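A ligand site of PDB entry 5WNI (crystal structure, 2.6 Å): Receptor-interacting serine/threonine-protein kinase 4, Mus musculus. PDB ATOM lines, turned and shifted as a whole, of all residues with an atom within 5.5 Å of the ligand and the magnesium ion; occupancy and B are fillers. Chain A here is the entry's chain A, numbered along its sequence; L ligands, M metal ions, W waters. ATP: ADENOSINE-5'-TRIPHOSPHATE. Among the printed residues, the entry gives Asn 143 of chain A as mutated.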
ATOM      1  N   VAL A  28     -20.034  19.660 -14.602  1.00  0.00           N
ATOM      2  CA  VAL A  28     -20.200  19.355 -13.178  1.00  0.00           C
ATOM      3  C   VAL A  28     -20.448  17.855 -12.927  1.00  0.00           C
ATOM      4  O   VAL A  28     -20.264  17.389 -11.803  1.00  0.00           O
ATOM      5  CB  VAL A  28     -21.330  20.219 -12.565  1.00  0.00           C
ATOM      6  CG1 VAL A  28     -21.459  19.982 -11.061  1.00  0.00           C
ATOM      7  CG2 VAL A  28     -21.067  21.693 -12.819  1.00  0.00           C
ATOM      8  N   GLY A  29     -20.820  17.086 -13.960  1.00  0.00           N
ATOM      9  CA  GLY A  29     -21.220  15.676 -13.807  1.00  0.00           C
ATOM     10  C   GLY A  29     -20.165  14.655 -13.395  1.00  0.00           C
ATOM     11  O   GLY A  29     -19.025  15.003 -13.046  1.00  0.00           O
ATOM     12  N   SER A  30     -20.567  13.386 -13.433  1.00  0.00           N
ATOM     13  CA  SER A  30     -19.758  12.303 -12.871  1.00  0.00           C
ATOM     14  C   SER A  30     -20.201  10.947 -13.433  1.00  0.00           C
ATOM     15  O   SER A  30     -21.392  10.643 -13.446  1.00  0.00           O
ATOM     16  CB  SER A  30     -19.901  12.300 -11.346  1.00  0.00           C
ATOM     17  OG  SER A  30     -19.063  11.334 -10.764  1.00  0.00           O
ATOM     18  N   GLN A  35     -23.364  12.882 -18.620  1.00  0.00           N
ATOM     19  CA  GLN A  35     -22.598  14.095 -18.384  1.00  0.00           C
ATOM     20  C   GLN A  35     -23.478  15.335 -18.140  1.00  0.00           C
ATOM     21  O   GLN A  35     -24.354  15.665 -18.964  1.00  0.00           O
ATOM     22  CB  GLN A  35     -21.651  14.384 -19.560  1.00  0.00           C
ATOM     23  CG  GLN A  35     -20.666  15.556 -19.365  1.00  0.00           C
ATOM     24  CD  GLN A  35     -19.644  15.348 -18.236  1.00  0.00           C
ATOM     25  OE1 GLN A  35     -19.114  14.253 -18.049  1.00  0.00           O
ATOM     26  NE2 GLN A  35     -19.367  16.410 -17.477  1.00  0.00           N
ATOM     27  N   VAL A  36     -23.182  16.041 -17.058  1.00  0.00           N
ATOM     28  CA  VAL A  36     -23.983  17.162 -16.548  1.00  0.00           C
ATOM     29  C   VAL A  36     -23.230  18.482 -16.643  1.00  0.00           C
ATOM     30  O   VAL A  36     -22.054  18.573 -16.250  1.00  0.00           O
ATOM     31  CB  VAL A  36     -24.404  16.906 -15.081  1.00  0.00           C
ATOM     32  CG1 VAL A  36     -25.063  18.147 -14.458  1.00  0.00           C
ATOM     33  CG2 VAL A  36     -25.332  15.712 -15.020  1.00  0.00           C
ATOM     34  N   ALA A  49     -29.051  23.618 -14.899  1.00  0.00           N
ATOM     35  CA  ALA A  49     -28.245  22.411 -15.081  1.00  0.00           C
ATOM     36  C   ALA A  49     -28.860  21.600 -16.192  1.00  0.00           C
ATOM     37  O   ALA A  49     -30.090  21.555 -16.322  1.00  0.00           O
ATOM     38  CB  ALA A  49     -28.217  21.585 -13.816  1.00  0.00           C
ATOM     39  N   LYS A  51     -28.452  17.682 -18.070  1.00  0.00           N
ATOM     40  CA  LYS A  51     -27.903  16.321 -18.046  1.00  0.00           C
ATOM     41  C   LYS A  51     -27.985  15.745 -19.462  1.00  0.00           C
ATOM     42  O   LYS A  51     -29.062  15.325 -19.903  1.00  0.00           O
ATOM     43  CB  LYS A  51     -28.684  15.414 -17.089  1.00  0.00           C
ATOM     44  CG  LYS A  51     -28.031  14.052 -16.822  1.00  0.00           C
ATOM     45  CD  LYS A  51     -29.020  12.908 -16.645  1.00  0.00           C
ATOM     46  CE  LYS A  51     -30.026  13.184 -15.548  1.00  0.00           C
ATOM     47  NZ  LYS A  51     -30.582  11.926 -14.973  1.00  0.00           N
ATOM     48  N   GLU A  69     -38.423  10.663 -17.350  1.00  0.00           N
ATOM     49  CA  GLU A  69     -37.691  11.179 -16.201  1.00  0.00           C
ATOM     50  C   GLU A  69     -38.187  12.589 -15.847  1.00  0.00           C
ATOM     51  O   GLU A  69     -38.621  12.817 -14.728  1.00  0.00           O
ATOM     52  CB  GLU A  69     -36.184  11.160 -16.479  1.00  0.00           C
ATOM     53  CG  GLU A  69     -35.334  11.549 -15.284  1.00  0.00           C
ATOM     54  CD  GLU A  69     -33.844  11.290 -15.472  1.00  0.00           C
ATOM     55  OE1 GLU A  69     -33.469  10.516 -16.381  1.00  0.00           O
ATOM     56  OE2 GLU A  69     -33.044  11.846 -14.687  1.00  0.00           O
ATOM     57  N   LEU A  82     -35.908  18.035  -6.760  1.00  0.00           N
ATOM     58  CA  LEU A  82     -35.312  18.997  -7.704  1.00  0.00           C
ATOM     59  C   LEU A  82     -36.341  19.425  -8.737  1.00  0.00           C
ATOM     60  O   LEU A  82     -36.976  18.569  -9.346  1.00  0.00           O
ATOM     61  CB  LEU A  82     -34.102  18.397  -8.425  1.00  0.00           C
ATOM     62  CG  LEU A  82     -33.273  19.412  -9.241  1.00  0.00           C
ATOM     63  CD1 LEU A  82     -32.511  20.400  -8.356  1.00  0.00           C
ATOM     64  CD2 LEU A  82     -32.320  18.658 -10.137  1.00  0.00           C
ATOM     65  N   MET A  96     -32.810  21.429 -15.822  1.00  0.00           N
ATOM     66  CA  MET A  96     -33.265  21.470 -14.420  1.00  0.00           C
ATOM     67  C   MET A  96     -32.609  22.552 -13.547  1.00  0.00           C
ATOM     68  O   MET A  96     -31.597  23.151 -13.952  1.00  0.00           O
ATOM     69  CB  MET A  96     -33.039  20.083 -13.787  1.00  0.00           C
ATOM     70  CG  MET A  96     -31.583  19.647 -13.777  1.00  0.00           C
ATOM     71  SD  MET A  96     -31.378  17.885 -13.486  1.00  0.00           S
ATOM     72  CE  MET A  96     -29.663  17.684 -13.954  1.00  0.00           C
ATOM     73  N   GLU A  97     -33.144  22.777 -12.338  1.00  0.00           N
ATOM     74  CA  GLU A  97     -32.552  23.764 -11.412  1.00  0.00           C
ATOM     75  C   GLU A  97     -31.104  23.347 -11.112  1.00  0.00           C
ATOM     76  O   GLU A  97     -30.782  22.151 -10.995  1.00  0.00           O
ATOM     77  CB  GLU A  97     -33.374  23.971 -10.108  1.00  0.00           C
ATOM     78  CG  GLU A  97     -33.821  25.431  -9.798  1.00  0.00           C
ATOM     79  N   TYR A  98     -30.224  24.356 -11.048  1.00  0.00           N
ATOM     80  CA  TYR A  98     -28.830  24.165 -10.728  1.00  0.00           C
ATOM     81  C   TYR A  98     -28.685  24.266  -9.234  1.00  0.00           C
ATOM     82  O   TYR A  98     -29.132  25.235  -8.620  1.00  0.00           O
ATOM     83  CB  TYR A  98     -27.945  25.230 -11.382  1.00  0.00           C
ATOM     84  CG  TYR A  98     -26.462  25.090 -11.027  1.00  0.00           C
ATOM     85  CD1 TYR A  98     -25.769  23.917 -11.322  1.00  0.00           C
ATOM     86  CD2 TYR A  98     -25.769  26.114 -10.393  1.00  0.00           C
ATOM     87  CE1 TYR A  98     -24.423  23.779 -10.993  1.00  0.00           C
ATOM     88  CE2 TYR A  98     -24.426  25.989 -10.067  1.00  0.00           C
ATOM     89  CZ  TYR A  98     -23.759  24.824 -10.369  1.00  0.00           C
ATOM     90  OH  TYR A  98     -22.436  24.690 -10.034  1.00  0.00           O
ATOM     91  N   MET A  99     -28.008  23.286  -8.661  1.00  0.00           N
ATOM     92  CA  MET A  99     -27.749  23.240  -7.243  1.00  0.00           C
ATOM     93  C   MET A  99     -26.264  23.553  -7.038  1.00  0.00           C
ATOM     94  O   MET A  99     -25.395  22.761  -7.415  1.00  0.00           O
ATOM     95  CB  MET A  99     -28.141  21.854  -6.714  1.00  0.00           C
ATOM     96  CG  MET A  99     -29.624  21.507  -6.935  1.00  0.00           C
ATOM     97  SD  MET A  99     -30.746  22.512  -5.927  1.00  0.00           S
ATOM     98  CE  MET A  99     -30.451  21.677  -4.386  1.00  0.00           C
ATOM     99  N   GLY A 102     -23.905  21.035  -5.123  1.00  0.00           N
ATOM    100  CA  GLY A 102     -23.744  19.760  -5.790  1.00  0.00           C
ATOM    101  C   GLY A 102     -24.220  18.569  -4.980  1.00  0.00           C
ATOM    102  O   GLY A 102     -25.094  18.682  -4.139  1.00  0.00           O
ATOM    103  N   SER A 103     -23.603  17.418  -5.222  1.00  0.00           N
ATOM    104  CA  SER A 103     -24.095  16.184  -4.664  1.00  0.00           C
ATOM    105  C   SER A 103     -23.648  16.007  -3.210  1.00  0.00           C
ATOM    106  O   SER A 103     -22.635  16.570  -2.773  1.00  0.00           O
ATOM    107  CB  SER A 103     -23.597  15.006  -5.502  1.00  0.00           C
ATOM    108  OG  SER A 103     -22.200  14.808  -5.318  1.00  0.00           O
ATOM    109  N   GLU A 105     -22.555  13.102  -2.225  1.00  0.00           N
ATOM    110  CA  GLU A 105     -21.371  12.256  -2.355  1.00  0.00           C
ATOM    111  C   GLU A 105     -20.116  13.109  -2.298  1.00  0.00           C
ATOM    112  O   GLU A 105     -19.175  12.831  -1.523  1.00  0.00           O
ATOM    113  CB  GLU A 105     -21.405  11.445  -3.659  1.00  0.00           C
ATOM    114  CG  GLU A 105     -20.057  10.861  -4.074  1.00  0.00           C
ATOM    115  CD  GLU A 105     -20.185   9.876  -5.208  1.00  0.00           C
ATOM    116  OE1 GLU A 105     -20.641  10.294  -6.299  1.00  0.00           O
ATOM    117  OE2 GLU A 105     -19.836   8.685  -5.015  1.00  0.00           O
ATOM    118  N   ASN A 143     -33.249   4.658  -6.980  1.00  0.00           N
ATOM    119  CA  ASN A 143     -31.869   5.019  -7.223  1.00  0.00           C
ATOM    120  C   ASN A 143     -31.370   6.017  -6.160  1.00  0.00           C
ATOM    121  O   ASN A 143     -30.581   6.916  -6.449  1.00  0.00           O
ATOM    122  CB  ASN A 143     -31.778   5.604  -8.631  1.00  0.00           C
ATOM    123  CG  ASN A 143     -30.380   5.557  -9.225  1.00  0.00           C
ATOM    124  OD1 ASN A 143     -29.495   4.764  -8.809  1.00  0.00           O
ATOM    125  ND2 ASN A 143     -30.169   6.404 -10.214  1.00  0.00           N
ATOM    126  N   LYS A 145     -29.119   7.329  -3.659  1.00  0.00           N
ATOM    127  CA  LYS A 145     -27.742   7.258  -3.165  1.00  0.00           C
ATOM    128  C   LYS A 145     -27.200   8.691  -3.019  1.00  0.00           C
ATOM    129  O   LYS A 145     -27.772   9.630  -3.575  1.00  0.00           O
ATOM    130  CB  LYS A 145     -26.878   6.379  -4.090  1.00  0.00           C
ATOM    131  CG  LYS A 145     -26.988   6.627  -5.594  1.00  0.00           C
ATOM    132  CD  LYS A 145     -26.345   5.482  -6.370  1.00  0.00           C
ATOM    133  CE  LYS A 145     -25.921   5.903  -7.785  1.00  0.00           C
ATOM    134  N   ALA A 147     -24.939  10.321  -4.443  1.00  0.00           N
ATOM    135  CA  ALA A 147     -24.716  10.998  -5.757  1.00  0.00           C
ATOM    136  C   ALA A 147     -25.974  11.668  -6.366  1.00  0.00           C
ATOM    137  O   ALA A 147     -25.838  12.549  -7.202  1.00  0.00           O
ATOM    138  CB  ALA A 147     -24.107  10.027  -6.768  1.00  0.00           C
ATOM    139  N   ASN A 148     -27.159  11.237  -5.955  1.00  0.00           N
ATOM    140  CA  ASN A 148     -28.440  11.747  -6.445  1.00  0.00           C
ATOM    141  C   ASN A 148     -29.197  12.608  -5.424  1.00  0.00           C
ATOM    142  O   ASN A 148     -30.401  12.877  -5.600  1.00  0.00           O
ATOM    143  CB  ASN A 148     -29.338  10.569  -6.864  1.00  0.00           C
ATOM    144  CG  ASN A 148     -28.720   9.732  -7.966  1.00  0.00           C
ATOM    145  OD1 ASN A 148     -27.898  10.201  -8.780  1.00  0.00           O
ATOM    146  ND2 ASN A 148     -29.134   8.476  -8.028  1.00  0.00           N
ATOM    147  N   LEU A 150     -28.996  16.212  -3.996  1.00  0.00           N
ATOM    148  CA  LEU A 150     -28.356  17.470  -4.338  1.00  0.00           C
ATOM    149  C   LEU A 150     -28.586  18.510  -3.254  1.00  0.00           C
ATOM    150  O   LEU A 150     -29.550  18.446  -2.491  1.00  0.00           O
ATOM    151  CB  LEU A 150     -28.812  17.964  -5.695  1.00  0.00           C
ATOM    152  CG  LEU A 150     -28.574  16.974  -6.874  1.00  0.00           C
ATOM    153  CD1 LEU A 150     -29.168  17.505  -8.181  1.00  0.00           C
ATOM    154  CD2 LEU A 150     -27.096  16.675  -7.061  1.00  0.00           C
ATOM    155  N   SER A 160     -32.848  14.067  -6.629  1.00  0.00           N
ATOM    156  CA  SER A 160     -32.848  14.081  -8.087  1.00  0.00           C
ATOM    157  C   SER A 160     -32.686  12.672  -8.644  1.00  0.00           C
ATOM    158  O   SER A 160     -32.745  11.726  -7.885  1.00  0.00           O
ATOM    159  CB  SER A 160     -31.700  14.979  -8.568  1.00  0.00           C
ATOM    160  OG  SER A 160     -31.987  15.447  -9.874  1.00  0.00           O
ATOM    161  N   ASP A 161     -32.480  12.581  -9.959  1.00  0.00           N
ATOM    162  CA  ASP A 161     -32.208  11.340 -10.697  1.00  0.00           C
ATOM    163  C   ASP A 161     -33.357  10.367 -10.621  1.00  0.00           C
ATOM    164  O   ASP A 161     -33.356   9.418  -9.833  1.00  0.00           O
ATOM    165  CB  ASP A 161     -30.887  10.679 -10.266  1.00  0.00           C
ATOM    166  CG  ASP A 161     -30.315   9.694 -11.354  1.00  0.00           C
ATOM    167  OD1 ASP A 161     -30.975   9.468 -12.402  1.00  0.00           O
ATOM    168  OD2 ASP A 161     -29.180   9.154 -11.155  1.00  0.00           O
ATOM    169  N   GLY A 163     -34.368   8.574 -13.353  1.00  0.00           N
ATOM    170  CA  GLY A 163     -34.223   7.604 -14.446  1.00  0.00           C
ATOM    171  C   GLY A 163     -34.791   6.225 -14.163  1.00  0.00           C
ATOM    172  O   GLY A 163     -35.331   5.601 -15.063  1.00  0.00           O
HETATM  173  PG  ATP L   1     -28.971   8.362 -15.212  1.00  0.00           P
HETATM  174  O1G ATP L   1     -30.363   8.765 -15.685  1.00  0.00           O
HETATM  175  O2G ATP L   1     -28.095   7.841 -16.340  1.00  0.00           O
HETATM  176  O3G ATP L   1     -29.033   7.392 -14.026  1.00  0.00           O
HETATM  177  PB  ATP L   1     -26.802  10.239 -14.171  1.00  0.00           P
HETATM  178  O1B ATP L   1     -26.522   9.548 -12.854  1.00  0.00           O
HETATM  179  O2B ATP L   1     -25.807  10.174 -15.283  1.00  0.00           O
HETATM  180  O3B ATP L   1     -28.256   9.755 -14.691  1.00  0.00           O
HETATM  181  PA  ATP L   1     -27.424  12.451 -12.402  1.00  0.00           P
HETATM  182  O1A ATP L   1     -28.171  13.717 -12.646  1.00  0.00           O
HETATM  183  O2A ATP L   1     -28.081  11.385 -11.571  1.00  0.00           O
HETATM  184  O3A ATP L   1     -27.056  11.783 -13.815  1.00  0.00           O
HETATM  185  O5' ATP L   1     -25.995  12.747 -11.703  1.00  0.00           O
HETATM  186  C5' ATP L   1     -24.914  13.474 -12.318  1.00  0.00           C
HETATM  187  C4' ATP L   1     -24.071  14.180 -11.272  1.00  0.00           C
HETATM  188  O4' ATP L   1     -23.965  15.578 -11.676  1.00  0.00           O
HETATM  189  C3' ATP L   1     -24.588  14.238  -9.814  1.00  0.00           C
HETATM  190  O3' ATP L   1     -24.077  13.195  -8.992  1.00  0.00           O
HETATM  191  C2' ATP L   1     -24.068  15.601  -9.335  1.00  0.00           C
HETATM  192  O2' ATP L   1     -22.716  15.595  -8.940  1.00  0.00           O
HETATM  193  C1' ATP L   1     -24.235  16.443 -10.600  1.00  0.00           C
HETATM  194  N9  ATP L   1     -25.589  17.032 -10.809  1.00  0.00           N
HETATM  195  C8  ATP L   1     -26.725  16.393 -11.263  1.00  0.00           C
HETATM  196  N7  ATP L   1     -27.759  17.193 -11.329  1.00  0.00           N
HETATM  197  C5  ATP L   1     -27.284  18.427 -10.876  1.00  0.00           C
HETATM  198  C6  ATP L   1     -27.901  19.680 -10.700  1.00  0.00           C
HETATM  199  N6  ATP L   1     -29.186  19.911 -10.956  1.00  0.00           N
HETATM  200  N1  ATP L   1     -27.139  20.697 -10.226  1.00  0.00           N
HETATM  201  C2  ATP L   1     -25.834  20.455  -9.971  1.00  0.00           C
HETATM  202  N3  ATP L   1     -25.152  19.321 -10.090  1.00  0.00           N
HETATM  203  C4  ATP L   1     -25.946  18.329 -10.558  1.00  0.00           C
HETATM  204 MG    MG M   1     -27.074   9.604 -10.733  1.00  0.00          MG
HETATM  205  O   HOH W   1     -21.461  17.625  -7.450  1.00  0.00           O
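The backbone carbonyl oxygen (O) of Ala 147 sits at hydrogen-bond distance from an oxygen (O3') of the ligand. O of Glu 97 is in hydrogen-bond range of N6 of the ligand, 2.8 Å away. The side-chain amino group (NZ) of Lys 51 is in salt-bridge range of an oxygen (O1G) of the ligand. The backbone NH (N) of Met 99 lies within hydrogen-bond range of a nitrogen (N1) of the ligand (3.1 Å).
The side-chain amino group (NZ) of Lys 51 lies within salt-bridge range of the side-chain carboxylate (OE2) of Glu 69. The side-chain amino group of Lys 51 is in salt-bridge range of the side-chain carboxylate of Asp 161 (3.6 Å). O of Val 36 lies within hydrogen-bond range of N of Val 28. The backbone carbonyl oxygen (O) of Asn 148 sits at hydrogen-bond distance from the backbone NH (N) of Ser 160 (2.9 Å). The side-chain carboxylate of Asp 161 lies close to the side-chain amide nitrogen of Asn 143. The backbone carbonyl oxygen (O) of Met 96 is in hydrogen-bond range of the backbone NH (N) of Ala 49, 2.8 Å away. N of Gly 29 sits at hydrogen-bond distance from O of Val 36. The side-chain amide nitrogen of Asn 148 lies within hydrogen-bond range of the backbone carbonyl oxygen of Asn 143, 2.6 Å away.
Residues that only touch the ligand: Met 96 (3.3 Å), Leu 150 (3.4 Å), Ala 49 (3.5 Å), Leu 82 (3.5 Å), Gly 29 (3.5 Å), Val 36 (3.5 Å), Ser 103 (3.6 Å), Glu 69 (3.6 Å), Tyr 98 (3.7 Å) and Val 28 (3.9 Å). Hydrophobic or aromatic side chains that line the ligand: Val 28, Val 36, Ala 49, Leu 82, Met 96, Tyr 98, Met 99, Ala 147 and Leu 150.
The magnesium ion is bound by an oxygen (O1B) of the ligand, the side-chain carboxylate of Asp 161, the side-chain amide oxygen of Asn 148 and an oxygen (O2A) of the ligand. The magnesium ion has four donor atoms within binding distance.
Water W1 bridges O2' of the ligand (2.8 Å) and N of Ser 103 (3.1 Å).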
